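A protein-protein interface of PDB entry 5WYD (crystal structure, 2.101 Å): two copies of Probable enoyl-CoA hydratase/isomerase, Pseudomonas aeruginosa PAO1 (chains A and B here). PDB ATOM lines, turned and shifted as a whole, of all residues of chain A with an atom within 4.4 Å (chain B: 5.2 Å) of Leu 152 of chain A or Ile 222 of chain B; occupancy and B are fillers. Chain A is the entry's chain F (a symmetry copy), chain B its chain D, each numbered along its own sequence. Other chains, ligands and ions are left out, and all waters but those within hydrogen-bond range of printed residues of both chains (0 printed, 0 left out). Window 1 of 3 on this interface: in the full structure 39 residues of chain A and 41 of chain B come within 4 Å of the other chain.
Leu 152 of chain A touches six residues of chain B.
Of chain A, only Leu 152 (3.3 Å), Ile 174 (3.4 Å) and Leu 175 (3.6 Å) come within 4 Å of Ile 222 of chain B.
Printed residues of chain B within 4 Å of Gly 150 of chain A: Ala 218 (3.5 Å) and Leu 248 (3.7 Å).
Of the printed residues of chain B, Cys 154 of chain A touches Glu 241 and Phe 245.
Printed residues of chain A within 4 Å of Leu 225 of chain B: Leu 152 (3.5 Å).
Of the printed residues of chain A, Ile 226 of chain B touches Ile 174 (3.4 Å) and Leu 175 (3.7 Å).
Thr 221 of chain B touches none of the printed residues of chain A.
The nearest printed residue of chain A that does not touch Ile 222 of chain B is Pro 153 of chain A (4.8 Å).
The nearest printed residue of chain B that does not touch Gly 150 of chain A is Ile 222 of chain B (5.6 Å).
Of the 13 printed residues of chain B, 9 touch a printed residue of chain A.
Hydrophobic or aromatic side chains of chain B within 4 Å of the printed part of chain A: Ala 218, Ile 219, Ile 222, Leu 225, Ile 226, Phe 245 and Leu 248.
Hydrophobic or aromatic side chains of chain A that line the printed part of chain B: Leu 152, Ile 174 and Leu 175.
Among the printed residues, 16 pairs touch across the chains.
No position is printed for both chains.
The backbone carbonyl oxygen (O) of Cys 154 of chain A sits close to the side-chain carboxylate (OE1) of Glu 241 of chain B.
The side-chain carboxylate of Glu 241 of chain B lies close to the backbone carbonyl oxygen of Pro 153 of chain A.
Among the printed residues, pairs that only touch across the chains: Leu 152 of chain A with Phe 245 of chain B (3.1 Å), Leu 152 of chain A with Ile 222 of chain B (3.3 Å), Ile 174 of chain A with Ile 222 of chain B (3.4 Å), Ile 174 of chain A with Ile 226 of chain B (3.4 Å), Cys 154 of chain A with Phe 245 of chain B (3.5 Å), Gly 150 of chain A with Ala 218 of chain B (3.5 Å), Leu 152 of chain A with Leu 225 of chain B (3.5 Å), Leu 152 of chain A with Glu 241 of chain B (3.6 Å), Leu 175 of chain A with Ile 222 of chain B (3.6 Å), Leu 152 of chain A with Leu 248 of chain B (3.7 Å), Gly 150 of chain A with Leu 248 of chain B (3.7 Å), Leu 175 of chain A with Ile 226 of chain B (3.7 Å), Leu 175 of chain A with Ile 219 of chain B (3.7 Å) and Leu 152 of chain A with Arg 244 of chain B (3.8 Å).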
ATOM      1  N   GLU A 146     -14.865  27.690  25.706  1.00  0.00           N
ATOM      2  CA  GLU A 146     -15.579  26.526  25.230  1.00  0.00           C
ATOM      3  C   GLU A 146     -16.978  26.891  24.771  1.00  0.00           C
ATOM      4  O   GLU A 146     -17.507  26.252  23.869  1.00  0.00           O
ATOM      5  CB  GLU A 146     -15.568  25.465  26.323  1.00  0.00           C
ATOM      6  CG  GLU A 146     -15.208  25.992  27.660  1.00  0.00           C
ATOM      7  CD  GLU A 146     -13.759  25.827  27.954  1.00  0.00           C
ATOM      8  OE1 GLU A 146     -13.173  26.767  28.471  1.00  0.00           O
ATOM      9  OE2 GLU A 146     -13.187  24.779  27.653  1.00  0.00           O
ATOM     10  N   GLY A 150     -19.376  25.964  21.307  1.00  0.00           N
ATOM     11  CA  GLY A 150     -20.524  25.135  21.602  1.00  0.00           C
ATOM     12  C   GLY A 150     -20.290  23.982  22.552  1.00  0.00           C
ATOM     13  O   GLY A 150     -21.194  23.144  22.687  1.00  0.00           O
ATOM     14  N   LEU A 151     -19.116  23.938  23.211  1.00  0.00           N
ATOM     15  CA  LEU A 151     -18.651  22.882  24.110  1.00  0.00           C
ATOM     16  C   LEU A 151     -18.571  23.422  25.524  1.00  0.00           C
ATOM     17  O   LEU A 151     -18.156  24.549  25.708  1.00  0.00           O
ATOM     18  CB  LEU A 151     -17.266  22.396  23.701  1.00  0.00           C
ATOM     19  CG  LEU A 151     -17.211  21.791  22.307  1.00  0.00           C
ATOM     20  CD1 LEU A 151     -15.816  21.254  21.955  1.00  0.00           C
ATOM     21  CD2 LEU A 151     -18.283  20.742  22.185  1.00  0.00           C
ATOM     22  N   LEU A 152     -19.079  22.715  26.485  1.00  0.00           N
ATOM     23  CA  LEU A 152     -18.867  23.235  27.837  1.00  0.00           C
ATOM     24  C   LEU A 152     -17.543  22.782  28.466  1.00  0.00           C
ATOM     25  O   LEU A 152     -16.952  21.783  28.049  1.00  0.00           O
ATOM     26  CB  LEU A 152     -20.027  22.837  28.701  1.00  0.00           C
ATOM     27  CG  LEU A 152     -20.437  21.398  28.844  1.00  0.00           C
ATOM     28  CD1 LEU A 152     -19.446  20.598  29.670  1.00  0.00           C
ATOM     29  CD2 LEU A 152     -21.875  21.390  29.376  1.00  0.00           C
ATOM     30  N   PRO A 153     -17.049  23.511  29.461  1.00  0.00           N
ATOM     31  CA  PRO A 153     -15.886  23.022  30.214  1.00  0.00           C
ATOM     32  C   PRO A 153     -16.286  21.734  30.915  1.00  0.00           C
ATOM     33  O   PRO A 153     -17.222  21.724  31.705  1.00  0.00           O
ATOM     34  CB  PRO A 153     -15.650  24.129  31.241  1.00  0.00           C
ATOM     35  CG  PRO A 153     -16.289  25.318  30.687  1.00  0.00           C
ATOM     36  CD  PRO A 153     -17.483  24.840  29.912  1.00  0.00           C
ATOM     37  N   CYS A 154     -15.557  20.650  30.686  1.00  0.00           N
ATOM     38  CA  CYS A 154     -15.979  19.390  31.292  1.00  0.00           C
ATOM     39  C   CYS A 154     -15.052  18.974  32.408  1.00  0.00           C
ATOM     40  O   CYS A 154     -15.160  17.855  32.918  1.00  0.00           O
ATOM     41  CB  CYS A 154     -15.997  18.269  30.274  1.00  0.00           C
ATOM     42  SG  CYS A 154     -14.324  17.957  29.776  1.00  0.00           S
ATOM     43  N   ILE A 174     -17.289  32.665  30.899  1.00  0.00           N
ATOM     44  CA  ILE A 174     -17.751  31.524  30.119  1.00  0.00           C
ATOM     45  C   ILE A 174     -18.912  31.883  29.191  1.00  0.00           C
ATOM     46  O   ILE A 174     -18.850  31.627  27.988  1.00  0.00           O
ATOM     47  CB  ILE A 174     -18.080  30.350  31.053  1.00  0.00           C
ATOM     48  CG1 ILE A 174     -18.437  29.128  30.216  1.00  0.00           C
ATOM     49  CG2 ILE A 174     -19.086  30.723  32.114  1.00  0.00           C
ATOM     50  CD1 ILE A 174     -18.758  27.947  31.055  1.00  0.00           C
ATOM     51  N   LEU A 175     -19.997  32.435  29.729  1.00  0.00           N
ATOM     52  CA  LEU A 175     -21.147  32.785  28.900  1.00  0.00           C
ATOM     53  C   LEU A 175     -20.822  33.939  27.956  1.00  0.00           C
ATOM     54  O   LEU A 175     -21.223  33.910  26.790  1.00  0.00           O
ATOM     55  CB  LEU A 175     -22.377  33.050  29.796  1.00  0.00           C
ATOM     56  CG  LEU A 175     -23.347  31.868  30.097  1.00  0.00           C
ATOM     57  CD1 LEU A 175     -22.641  30.594  30.446  1.00  0.00           C
ATOM     58  CD2 LEU A 175     -24.270  32.243  31.263  1.00  0.00           C
ATOM     59  N   ALA B 218     -25.450  25.695  23.347  1.00  0.00           N
ATOM     60  CA  ALA B 218     -24.455  25.606  24.423  1.00  0.00           C
ATOM     61  C   ALA B 218     -24.768  26.536  25.581  1.00  0.00           C
ATOM     62  O   ALA B 218     -24.807  26.099  26.738  1.00  0.00           O
ATOM     63  CB  ALA B 218     -23.057  25.940  23.922  1.00  0.00           C
ATOM     64  N   ILE B 219     -25.087  27.796  25.299  1.00  0.00           N
ATOM     65  CA  ILE B 219     -25.308  28.707  26.420  1.00  0.00           C
ATOM     66  C   ILE B 219     -26.419  28.163  27.312  1.00  0.00           C
ATOM     67  O   ILE B 219     -26.213  27.951  28.513  1.00  0.00           O
ATOM     68  CB  ILE B 219     -25.617  30.131  25.895  1.00  0.00           C
ATOM     69  CG1 ILE B 219     -24.445  30.677  25.101  1.00  0.00           C
ATOM     70  CG2 ILE B 219     -25.974  31.119  26.976  1.00  0.00           C
ATOM     71  CD1 ILE B 219     -23.191  30.850  25.902  1.00  0.00           C
ATOM     72  N   ARG B 220     -27.515  27.709  26.694  1.00  0.00           N
ATOM     73  CA  ARG B 220     -28.669  27.264  27.449  1.00  0.00           C
ATOM     74  C   ARG B 220     -28.309  26.125  28.383  1.00  0.00           C
ATOM     75  O   ARG B 220     -28.851  26.034  29.483  1.00  0.00           O
ATOM     76  CB  ARG B 220     -29.811  26.858  26.509  1.00  0.00           C
ATOM     77  CG  ARG B 220     -30.004  27.719  25.344  1.00  0.00           C
ATOM     78  CD  ARG B 220     -31.247  27.283  24.624  1.00  0.00           C
ATOM     79  NE  ARG B 220     -31.205  27.657  23.217  1.00  0.00           N
ATOM     80  CZ  ARG B 220     -31.598  28.834  22.738  1.00  0.00           C
ATOM     81  NH1 ARG B 220     -32.042  29.789  23.550  1.00  0.00           N
ATOM     82  NH2 ARG B 220     -31.519  29.064  21.436  1.00  0.00           N
ATOM     83  N   THR B 221     -27.519  25.171  27.919  1.00  0.00           N
ATOM     84  CA  THR B 221     -27.163  24.072  28.810  1.00  0.00           C
ATOM     85  C   THR B 221     -26.102  24.458  29.845  1.00  0.00           C
ATOM     86  O   THR B 221     -26.110  23.922  30.959  1.00  0.00           O
ATOM     87  CB  THR B 221     -26.774  22.828  28.013  1.00  0.00           C
ATOM     88  OG1 THR B 221     -26.191  21.860  28.891  1.00  0.00           O
ATOM     89  CG2 THR B 221     -25.831  23.134  26.921  1.00  0.00           C
ATOM     90  N   ILE B 222     -25.132  25.303  29.486  1.00  0.00           N
ATOM     91  CA  ILE B 222     -24.073  25.607  30.451  1.00  0.00           C
ATOM     92  C   ILE B 222     -24.600  26.371  31.679  1.00  0.00           C
ATOM     93  O   ILE B 222     -24.181  26.117  32.825  1.00  0.00           O
ATOM     94  CB  ILE B 222     -22.938  26.388  29.764  1.00  0.00           C
ATOM     95  CG1 ILE B 222     -22.089  25.531  28.795  1.00  0.00           C
ATOM     96  CG2 ILE B 222     -22.035  27.053  30.831  1.00  0.00           C
ATOM     97  CD1 ILE B 222     -22.694  24.589  27.911  1.00  0.00           C
ATOM     98  N   LYS B 223     -25.520  27.311  31.469  1.00  0.00           N
ATOM     99  CA  LYS B 223     -25.942  28.171  32.574  1.00  0.00           C
ATOM    100  C   LYS B 223     -26.447  27.376  33.770  1.00  0.00           C
ATOM    101  O   LYS B 223     -26.145  27.771  34.908  1.00  0.00           O
ATOM    102  CB  LYS B 223     -27.030  29.139  32.090  1.00  0.00           C
ATOM    103  CG  LYS B 223     -27.493  30.231  33.066  1.00  0.00           C
ATOM    104  CD  LYS B 223     -28.673  31.006  32.392  1.00  0.00           C
ATOM    105  CE  LYS B 223     -29.156  32.261  33.118  1.00  0.00           C
ATOM    106  NZ  LYS B 223     -29.789  32.095  34.432  1.00  0.00           N
ATOM    107  N   PRO B 224     -27.196  26.283  33.614  1.00  0.00           N
ATOM    108  CA  PRO B 224     -27.608  25.530  34.809  1.00  0.00           C
ATOM    109  C   PRO B 224     -26.443  24.986  35.588  1.00  0.00           C
ATOM    110  O   PRO B 224     -26.484  24.987  36.819  1.00  0.00           O
ATOM    111  CB  PRO B 224     -28.466  24.406  34.236  1.00  0.00           C
ATOM    112  CG  PRO B 224     -29.071  25.013  33.007  1.00  0.00           C
ATOM    113  CD  PRO B 224     -28.039  25.950  32.454  1.00  0.00           C
ATOM    114  N   LEU B 225     -25.402  24.519  34.899  1.00  0.00           N
ATOM    115  CA  LEU B 225     -24.246  23.967  35.592  1.00  0.00           C
ATOM    116  C   LEU B 225     -23.603  24.992  36.505  1.00  0.00           C
ATOM    117  O   LEU B 225     -23.276  24.695  37.661  1.00  0.00           O
ATOM    118  CB  LEU B 225     -23.241  23.484  34.559  1.00  0.00           C
ATOM    119  CG  LEU B 225     -23.708  22.240  33.831  1.00  0.00           C
ATOM    120  CD1 LEU B 225     -22.692  21.765  32.805  1.00  0.00           C
ATOM    121  CD2 LEU B 225     -23.895  21.166  34.916  1.00  0.00           C
ATOM    122  N   ILE B 226     -23.463  26.220  36.015  1.00  0.00           N
ATOM    123  CA  ILE B 226     -22.873  27.277  36.823  1.00  0.00           C
ATOM    124  C   ILE B 226     -23.737  27.529  38.044  1.00  0.00           C
ATOM    125  O   ILE B 226     -23.237  27.620  39.174  1.00  0.00           O
ATOM    126  CB  ILE B 226     -22.727  28.543  35.963  1.00  0.00           C
ATOM    127  CG1 ILE B 226     -21.843  28.242  34.766  1.00  0.00           C
ATOM    128  CG2 ILE B 226     -22.142  29.697  36.757  1.00  0.00           C
ATOM    129  CD1 ILE B 226     -21.723  29.384  33.850  1.00  0.00           C
ATOM    130  N   GLU B 241     -21.526  17.068  34.740  1.00  0.00           N
ATOM    131  CA  GLU B 241     -20.839  17.984  33.836  1.00  0.00           C
ATOM    132  C   GLU B 241     -20.299  17.255  32.621  1.00  0.00           C
ATOM    133  O   GLU B 241     -20.457  17.717  31.486  1.00  0.00           O
ATOM    134  CB  GLU B 241     -19.698  18.668  34.557  1.00  0.00           C
ATOM    135  CG  GLU B 241     -19.045  19.751  33.746  1.00  0.00           C
ATOM    136  CD  GLU B 241     -17.768  20.252  34.376  1.00  0.00           C
ATOM    137  OE1 GLU B 241     -17.045  19.387  34.909  1.00  0.00           O
ATOM    138  OE2 GLU B 241     -17.505  21.482  34.373  1.00  0.00           O
ATOM    139  N   ARG B 244     -23.542  16.179  30.513  1.00  0.00           N
ATOM    140  CA  ARG B 244     -23.999  17.301  29.703  1.00  0.00           C
ATOM    141  C   ARG B 244     -23.049  17.533  28.553  1.00  0.00           C
ATOM    142  O   ARG B 244     -23.472  17.759  27.416  1.00  0.00           O
ATOM    143  CB  ARG B 244     -24.095  18.578  30.523  1.00  0.00           C
ATOM    144  CG  ARG B 244     -24.632  18.400  31.883  1.00  0.00           C
ATOM    145  CD  ARG B 244     -25.810  17.484  31.857  1.00  0.00           C
ATOM    146  NE  ARG B 244     -27.042  18.159  31.507  1.00  0.00           N
ATOM    147  CZ  ARG B 244     -28.239  17.642  31.744  1.00  0.00           C
ATOM    148  NH1 ARG B 244     -28.333  16.454  32.323  1.00  0.00           N
ATOM    149  NH2 ARG B 244     -29.337  18.306  31.409  1.00  0.00           N
ATOM    150  N   PHE B 245     -21.755  17.440  28.833  1.00  0.00           N
ATOM    151  CA  PHE B 245     -20.766  17.652  27.791  1.00  0.00           C
ATOM    152  C   PHE B 245     -20.977  16.669  26.651  1.00  0.00           C
ATOM    153  O   PHE B 245     -20.905  17.047  25.474  1.00  0.00           O
ATOM    154  CB  PHE B 245     -19.366  17.528  28.387  1.00  0.00           C
ATOM    155  CG  PHE B 245     -18.267  17.659  27.383  1.00  0.00           C
ATOM    156  CD1 PHE B 245     -17.889  16.583  26.594  1.00  0.00           C
ATOM    157  CD2 PHE B 245     -17.608  18.864  27.228  1.00  0.00           C
ATOM    158  CE1 PHE B 245     -16.876  16.702  25.676  1.00  0.00           C
ATOM    159  CE2 PHE B 245     -16.599  18.997  26.307  1.00  0.00           C
ATOM    160  CZ  PHE B 245     -16.224  17.910  25.531  1.00  0.00           C
ATOM    161  N   LEU B 248     -24.009  17.646  24.383  1.00  0.00           N
ATOM    162  CA  LEU B 248     -23.733  18.709  23.435  1.00  0.00           C
ATOM    163  C   LEU B 248     -23.132  18.137  22.185  1.00  0.00           C
ATOM    164  O   LEU B 248     -23.596  18.427  21.079  1.00  0.00           O
ATOM    165  CB  LEU B 248     -22.757  19.705  24.060  1.00  0.00           C
ATOM    166  CG  LEU B 248     -23.433  20.632  25.050  1.00  0.00           C
ATOM    167  CD1 LEU B 248     -22.461  21.540  25.754  1.00  0.00           C
ATOM    168  CD2 LEU B 248     -24.366  21.449  24.230  1.00  0.00           C
